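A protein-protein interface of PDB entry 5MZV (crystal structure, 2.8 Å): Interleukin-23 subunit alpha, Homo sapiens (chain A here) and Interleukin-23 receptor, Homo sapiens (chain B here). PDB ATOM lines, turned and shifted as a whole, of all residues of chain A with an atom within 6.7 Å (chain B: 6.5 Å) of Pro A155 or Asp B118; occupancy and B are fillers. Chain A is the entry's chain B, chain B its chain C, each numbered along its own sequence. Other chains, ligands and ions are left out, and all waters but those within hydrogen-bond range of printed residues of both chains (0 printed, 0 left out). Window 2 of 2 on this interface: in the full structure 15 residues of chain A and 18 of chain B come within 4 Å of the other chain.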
ATOM      1  N   GLU A 112      29.189   9.142 -33.213  1.00  0.00           N
ATOM      2  CA  GLU A 112      30.196   9.657 -32.294  1.00  0.00           C
ATOM      3  C   GLU A 112      29.527  10.262 -31.060  1.00  0.00           C
ATOM      4  O   GLU A 112      28.493  10.924 -31.180  1.00  0.00           O
ATOM      5  CB  GLU A 112      31.050  10.718 -32.983  1.00  0.00           C
ATOM      6  CG  GLU A 112      31.753  10.230 -34.238  1.00  0.00           C
ATOM      7  CD  GLU A 112      32.839   9.214 -33.940  1.00  0.00           C
ATOM      8  OE1 GLU A 112      33.306   9.162 -32.782  1.00  0.00           O
ATOM      9  OE2 GLU A 112      33.224   8.467 -34.864  1.00  0.00           O
ATOM     10  N   PRO A 113      30.095  10.069 -29.856  1.00  0.00           N
ATOM     11  CA  PRO A 113      31.302   9.289 -29.548  1.00  0.00           C
ATOM     12  C   PRO A 113      31.106   7.789 -29.738  1.00  0.00           C
ATOM     13  O   PRO A 113      30.002   7.281 -29.548  1.00  0.00           O
ATOM     14  CB  PRO A 113      31.571   9.622 -28.077  1.00  0.00           C
ATOM     15  CG  PRO A 113      30.266  10.066 -27.537  1.00  0.00           C
ATOM     16  CD  PRO A 113      29.575  10.759 -28.664  1.00  0.00           C
ATOM     17  N   SER A 153      20.330  12.828 -33.666  1.00  0.00           N
ATOM     18  CA  SER A 153      20.904  13.315 -32.421  1.00  0.00           C
ATOM     19  C   SER A 153      22.262  13.961 -32.657  1.00  0.00           C
ATOM     20  O   SER A 153      23.046  13.504 -33.494  1.00  0.00           O
ATOM     21  CB  SER A 153      21.048  12.173 -31.418  1.00  0.00           C
ATOM     22  OG  SER A 153      21.827  11.122 -31.963  1.00  0.00           O
ATOM     23  N   GLN A 154      22.532  15.029 -31.905  1.00  0.00           N
ATOM     24  CA  GLN A 154      23.830  15.678 -31.906  1.00  0.00           C
ATOM     25  C   GLN A 154      24.796  14.913 -31.003  1.00  0.00           C
ATOM     26  O   GLN A 154      24.388  14.354 -29.982  1.00  0.00           O
ATOM     27  CB  GLN A 154      23.709  17.120 -31.423  1.00  0.00           C
ATOM     28  CG  GLN A 154      23.360  18.127 -32.517  1.00  0.00           C
ATOM     29  CD  GLN A 154      22.116  17.747 -33.303  1.00  0.00           C
ATOM     30  OE1 GLN A 154      22.090  17.855 -34.529  1.00  0.00           O
ATOM     31  NE2 GLN A 154      21.074  17.312 -32.599  1.00  0.00           N
ATOM     32  N   PRO A 155      26.084  14.874 -31.354  1.00  0.00           N
ATOM     33  CA  PRO A 155      27.035  14.080 -30.555  1.00  0.00           C
ATOM     34  C   PRO A 155      26.961  14.322 -29.055  1.00  0.00           C
ATOM     35  O   PRO A 155      27.051  13.364 -28.279  1.00  0.00           O
ATOM     36  CB  PRO A 155      28.393  14.504 -31.129  1.00  0.00           C
ATOM     37  CG  PRO A 155      28.102  14.851 -32.539  1.00  0.00           C
ATOM     38  CD  PRO A 155      26.713  15.431 -32.565  1.00  0.00           C
ATOM     39  N   TRP A 156      26.794  15.573 -28.620  1.00  0.00           N
ATOM     40  CA  TRP A 156      26.866  15.866 -27.192  1.00  0.00           C
ATOM     41  C   TRP A 156      25.702  15.253 -26.420  1.00  0.00           C
ATOM     42  O   TRP A 156      25.829  14.996 -25.219  1.00  0.00           O
ATOM     43  CB  TRP A 156      26.914  17.377 -26.967  1.00  0.00           C
ATOM     44  CG  TRP A 156      25.667  18.112 -27.366  1.00  0.00           C
ATOM     45  CD1 TRP A 156      25.393  18.655 -28.585  1.00  0.00           C
ATOM     46  CD2 TRP A 156      24.529  18.396 -26.536  1.00  0.00           C
ATOM     47  NE1 TRP A 156      24.158  19.256 -28.570  1.00  0.00           N
ATOM     48  CE2 TRP A 156      23.608  19.112 -27.324  1.00  0.00           C
ATOM     49  CE3 TRP A 156      24.202  18.112 -25.207  1.00  0.00           C
ATOM     50  CZ2 TRP A 156      22.381  19.547 -26.829  1.00  0.00           C
ATOM     51  CZ3 TRP A 156      22.981  18.547 -24.717  1.00  0.00           C
ATOM     52  CH2 TRP A 156      22.087  19.257 -25.527  1.00  0.00           C
ATOM     53  N   GLN A 157      24.572  15.005 -27.083  1.00  0.00           N
ATOM     54  CA  GLN A 157      23.410  14.450 -26.398  1.00  0.00           C
ATOM     55  C   GLN A 157      23.539  12.954 -26.144  1.00  0.00           C
ATOM     56  O   GLN A 157      22.923  12.434 -25.207  1.00  0.00           O
ATOM     57  CB  GLN A 157      22.146  14.698 -27.223  1.00  0.00           C
ATOM     58  CG  GLN A 157      21.836  16.153 -27.484  1.00  0.00           C
ATOM     59  CD  GLN A 157      20.675  16.323 -28.437  1.00  0.00           C
ATOM     60  OE1 GLN A 157      20.418  15.461 -29.277  1.00  0.00           O
ATOM     61  NE2 GLN A 157      19.963  17.435 -28.310  1.00  0.00           N
ATOM     62  N   ARG A 158      24.338  12.253 -26.950  1.00  0.00           N
ATOM     63  CA  ARG A 158      24.186  10.806 -27.070  1.00  0.00           C
ATOM     64  C   ARG A 158      24.557  10.078 -25.782  1.00  0.00           C
ATOM     65  O   ARG A 158      23.880   9.119 -25.395  1.00  0.00           O
ATOM     66  CB  ARG A 158      25.012  10.309 -28.255  1.00  0.00           C
ATOM     67  CG  ARG A 158      24.480  10.849 -29.573  1.00  0.00           C
ATOM     68  CD  ARG A 158      25.365  10.520 -30.754  1.00  0.00           C
ATOM     69  NE  ARG A 158      24.869  11.159 -31.970  1.00  0.00           N
ATOM     70  CZ  ARG A 158      25.600  11.382 -33.056  1.00  0.00           C
ATOM     71  NH1 ARG A 158      26.875  11.025 -33.092  1.00  0.00           N
ATOM     72  NH2 ARG A 158      25.051  11.971 -34.110  1.00  0.00           N
ATOM     73  N   LEU A 159      25.619  10.505 -25.096  1.00  0.00           N
ATOM     74  CA  LEU A 159      25.961   9.856 -23.834  1.00  0.00           C
ATOM     75  C   LEU A 159      24.809   9.949 -22.843  1.00  0.00           C
ATOM     76  O   LEU A 159      24.546   9.001 -22.094  1.00  0.00           O
ATOM     77  CB  LEU A 159      27.228  10.470 -23.235  1.00  0.00           C
ATOM     78  CG  LEU A 159      28.570  10.116 -23.884  1.00  0.00           C
ATOM     79  CD1 LEU A 159      29.708  10.699 -23.054  1.00  0.00           C
ATOM     80  CD2 LEU A 159      28.754   8.611 -24.055  1.00  0.00           C
ATOM     81  N   LEU A 160      24.109  11.085 -22.826  1.00  0.00           N
ATOM     82  CA  LEU A 160      22.942  11.215 -21.961  1.00  0.00           C
ATOM     83  C   LEU A 160      21.784  10.368 -22.477  1.00  0.00           C
ATOM     84  O   LEU A 160      21.050   9.762 -21.688  1.00  0.00           O
ATOM     85  CB  LEU A 160      22.531  12.684 -21.854  1.00  0.00           C
ATOM     86  CG  LEU A 160      23.664  13.700 -21.643  1.00  0.00           C
ATOM     87  CD1 LEU A 160      23.112  15.116 -21.527  1.00  0.00           C
ATOM     88  CD2 LEU A 160      24.503  13.350 -20.416  1.00  0.00           C
ATOM     89  N   THR B  40      30.383  29.086 -33.114  1.00  0.00           N
ATOM     90  CA  THR B  40      30.510  27.678 -32.748  1.00  0.00           C
ATOM     91  C   THR B  40      31.557  26.980 -33.604  1.00  0.00           C
ATOM     92  O   THR B  40      32.162  26.000 -33.159  1.00  0.00           O
ATOM     93  CB  THR B  40      29.169  26.955 -32.877  1.00  0.00           C
ATOM     94  OG1 THR B  40      28.895  26.705 -34.257  1.00  0.00           O
ATOM     95  CG2 THR B  40      28.032  27.775 -32.264  1.00  0.00           C
ATOM     96  N   ILE B  41      31.769  27.456 -34.829  1.00  0.00           N
ATOM     97  CA  ILE B  41      32.894  27.044 -35.661  1.00  0.00           C
ATOM     98  C   ILE B  41      33.863  28.216 -35.711  1.00  0.00           C
ATOM     99  O   ILE B  41      33.483  29.330 -36.094  1.00  0.00           O
ATOM    100  CB  ILE B  41      32.451  26.631 -37.074  1.00  0.00           C
ATOM    101  CG1 ILE B  41      31.436  25.488 -37.002  1.00  0.00           C
ATOM    102  CG2 ILE B  41      33.663  26.210 -37.901  1.00  0.00           C
ATOM    103  CD1 ILE B  41      30.887  25.056 -38.345  1.00  0.00           C
ATOM    104  N   ASN B  69      33.217  17.462 -22.814  1.00  0.00           N
ATOM    105  CA  ASN B  69      33.372  16.023 -23.001  1.00  0.00           C
ATOM    106  C   ASN B  69      33.107  15.278 -21.698  1.00  0.00           C
ATOM    107  O   ASN B  69      33.775  14.295 -21.372  1.00  0.00           O
ATOM    108  CB  ASN B  69      34.761  15.690 -23.546  1.00  0.00           C
ATOM    109  CG  ASN B  69      35.007  16.297 -24.908  1.00  0.00           C
ATOM    110  OD1 ASN B  69      34.126  16.294 -25.768  1.00  0.00           O
ATOM    111  ND2 ASN B  69      36.205  16.831 -25.112  1.00  0.00           N
ATOM    112  N   HIS B  96      37.113  19.123 -32.403  1.00  0.00           N
ATOM    113  CA  HIS B  96      35.745  18.921 -31.952  1.00  0.00           C
ATOM    114  C   HIS B  96      35.730  18.929 -30.432  1.00  0.00           C
ATOM    115  O   HIS B  96      36.754  18.714 -29.780  1.00  0.00           O
ATOM    116  CB  HIS B  96      35.151  17.604 -32.475  1.00  0.00           C
ATOM    117  CG  HIS B  96      34.960  17.571 -33.959  1.00  0.00           C
ATOM    118  ND1 HIS B  96      34.137  18.457 -34.623  1.00  0.00           N
ATOM    119  CD2 HIS B  96      35.478  16.755 -34.908  1.00  0.00           C
ATOM    120  CE1 HIS B  96      34.162  18.191 -35.917  1.00  0.00           C
ATOM    121  NE2 HIS B  96      34.968  17.163 -36.116  1.00  0.00           N
ATOM    122  N   ALA B  97      34.551  19.185 -29.871  1.00  0.00           N
ATOM    123  CA  ALA B  97      34.373  19.165 -28.428  1.00  0.00           C
ATOM    124  C   ALA B  97      32.891  19.290 -28.118  1.00  0.00           C
ATOM    125  O   ALA B  97      32.195  20.107 -28.724  1.00  0.00           O
ATOM    126  CB  ALA B  97      35.154  20.298 -27.752  1.00  0.00           C
ATOM    127  N   SER B  98      32.417  18.478 -27.179  1.00  0.00           N
ATOM    128  CA  SER B  98      31.027  18.507 -26.748  1.00  0.00           C
ATOM    129  C   SER B  98      30.931  19.323 -25.467  1.00  0.00           C
ATOM    130  O   SER B  98      31.531  18.959 -24.450  1.00  0.00           O
ATOM    131  CB  SER B  98      30.497  17.092 -26.529  1.00  0.00           C
ATOM    132  OG  SER B  98      30.418  16.385 -27.753  1.00  0.00           O
ATOM    133  N   MET B  99      30.196  20.428 -25.524  1.00  0.00           N
ATOM    134  CA  MET B  99      29.980  21.291 -24.372  1.00  0.00           C
ATOM    135  C   MET B  99      28.553  21.124 -23.873  1.00  0.00           C
ATOM    136  O   MET B  99      27.627  20.932 -24.666  1.00  0.00           O
ATOM    137  CB  MET B  99      30.219  22.763 -24.724  1.00  0.00           C
ATOM    138  CG  MET B  99      31.600  23.076 -25.276  1.00  0.00           C
ATOM    139  SD  MET B  99      32.953  22.678 -24.154  1.00  0.00           S
ATOM    140  CE  MET B  99      32.493  23.584 -22.676  1.00  0.00           C
ATOM    141  N   GLY B 116      23.356  22.122 -24.368  1.00  0.00           N
ATOM    142  CA  GLY B 116      24.648  21.685 -24.857  1.00  0.00           C
ATOM    143  C   GLY B 116      24.846  22.064 -26.313  1.00  0.00           C
ATOM    144  O   GLY B 116      23.953  22.615 -26.954  1.00  0.00           O
ATOM    145  N   LYS B 117      26.035  21.758 -26.825  1.00  0.00           N
ATOM    146  CA  LYS B 117      26.380  22.191 -28.168  1.00  0.00           C
ATOM    147  C   LYS B 117      27.731  21.605 -28.533  1.00  0.00           C
ATOM    148  O   LYS B 117      28.638  21.572 -27.697  1.00  0.00           O
ATOM    149  CB  LYS B 117      26.431  23.723 -28.254  1.00  0.00           C
ATOM    150  CG  LYS B 117      26.629  24.267 -29.642  1.00  0.00           C
ATOM    151  CD  LYS B 117      26.658  25.784 -29.623  1.00  0.00           C
ATOM    152  CE  LYS B 117      25.273  26.383 -29.400  1.00  0.00           C
ATOM    153  NZ  LYS B 117      24.356  26.119 -30.535  1.00  0.00           N
ATOM    154  N   ASP B 118      27.854  21.155 -29.774  1.00  0.00           N
ATOM    155  CA  ASP B 118      29.121  20.689 -30.324  1.00  0.00           C
ATOM    156  C   ASP B 118      29.818  21.848 -31.018  1.00  0.00           C
ATOM    157  O   ASP B 118      29.227  22.516 -31.871  1.00  0.00           O
ATOM    158  CB  ASP B 118      28.901  19.554 -31.325  1.00  0.00           C
ATOM    159  CG  ASP B 118      28.528  18.255 -30.663  1.00  0.00           C
ATOM    160  OD1 ASP B 118      29.376  17.691 -29.941  1.00  0.00           O
ATOM    161  OD2 ASP B 118      27.386  17.798 -30.865  1.00  0.00           O
ATOM    162  N   ILE B 119      31.080  22.077 -30.662  1.00  0.00           N
ATOM    163  CA  ILE B 119      31.883  23.142 -31.249  1.00  0.00           C
ATOM    164  C   ILE B 119      32.988  22.511 -32.082  1.00  0.00           C
ATOM    165  O   ILE B 119      33.520  21.451 -31.732  1.00  0.00           O
ATOM    166  CB  ILE B 119      32.456  24.079 -30.170  1.00  0.00           C
ATOM    167  CG1 ILE B 119      33.440  23.345 -29.265  1.00  0.00           C
ATOM    168  CG2 ILE B 119      31.323  24.649 -29.335  1.00  0.00           C
ATOM    169  CD1 ILE B 119      34.181  24.262 -28.310  1.00  0.00           C
ATOM    170  N   SER B 120      33.318  23.158 -33.198  1.00  0.00           N
ATOM    171  CA  SER B 120      34.340  22.677 -34.111  1.00  0.00           C
ATOM    172  C   SER B 120      35.398  23.752 -34.307  1.00  0.00           C
ATOM    173  O   SER B 120      35.120  24.951 -34.200  1.00  0.00           O
ATOM    174  CB  SER B 120      33.738  22.294 -35.470  1.00  0.00           C
ATOM    175  OG  SER B 120      32.709  21.331 -35.325  1.00  0.00           O
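N of Trp A156 sits close to OD2 of Asp B118, 3.2 Å away.
OD2 of Asp B118 sits close to N of Pro A155.
The backbone NH of Gln A154 is in hydrogen-bond range of the side-chain amide oxygen of Gln A157 (3.4 Å).
The backbone carbonyl oxygen (O) of Met B99 is in hydrogen-bond range of the backbone NH (N) of Lys B117.
OD1 of Asp B118 lies within hydrogen-bond range of OG of Ser B98 (2.8 Å).
O of Ser B98 is in hydrogen-bond range of N of Asn B69, at 2.8 Å.
Asp B118 touches Gln A154 (OD2 to CB, 3.8 Å).
Ser B98 touches Trp A156.
Trp A156 touches Gly B116.
NE1 of Trp A156 touches N of Lys B117, at 3.6 Å.
Pro A113 touches none of the printed residues of chain B.
Printed residues of chain B within 4 Å of Gln A154: Asp B118 (3.8 Å).
Of chain B, only Asp B118 comes within 4 Å of Pro A155.
Of the printed residues of chain B, Trp A156 touches Ser B98, Gly B116, Lys B117 and Asp B118.
Arg A158 touches none of the printed residues of chain B.
Of the printed residues of chain A, Ser B98 touches Trp A156.
Of the printed residues of chain A, Gly B116 touches Trp A156.
Of chain A, only Gln A154, Pro A155 and Trp A156 come within 4 Å of Asp B118.
The nearest printed residue of chain A that does not touch Gly B116 is Gln A157 (6.7 Å).
Printed residues of chain B that touch a printed residue of chain A: Ser B98, Gly B116, Lys B117 and Asp B118.
Among the printed residues, 6 pairs touch across the chains.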
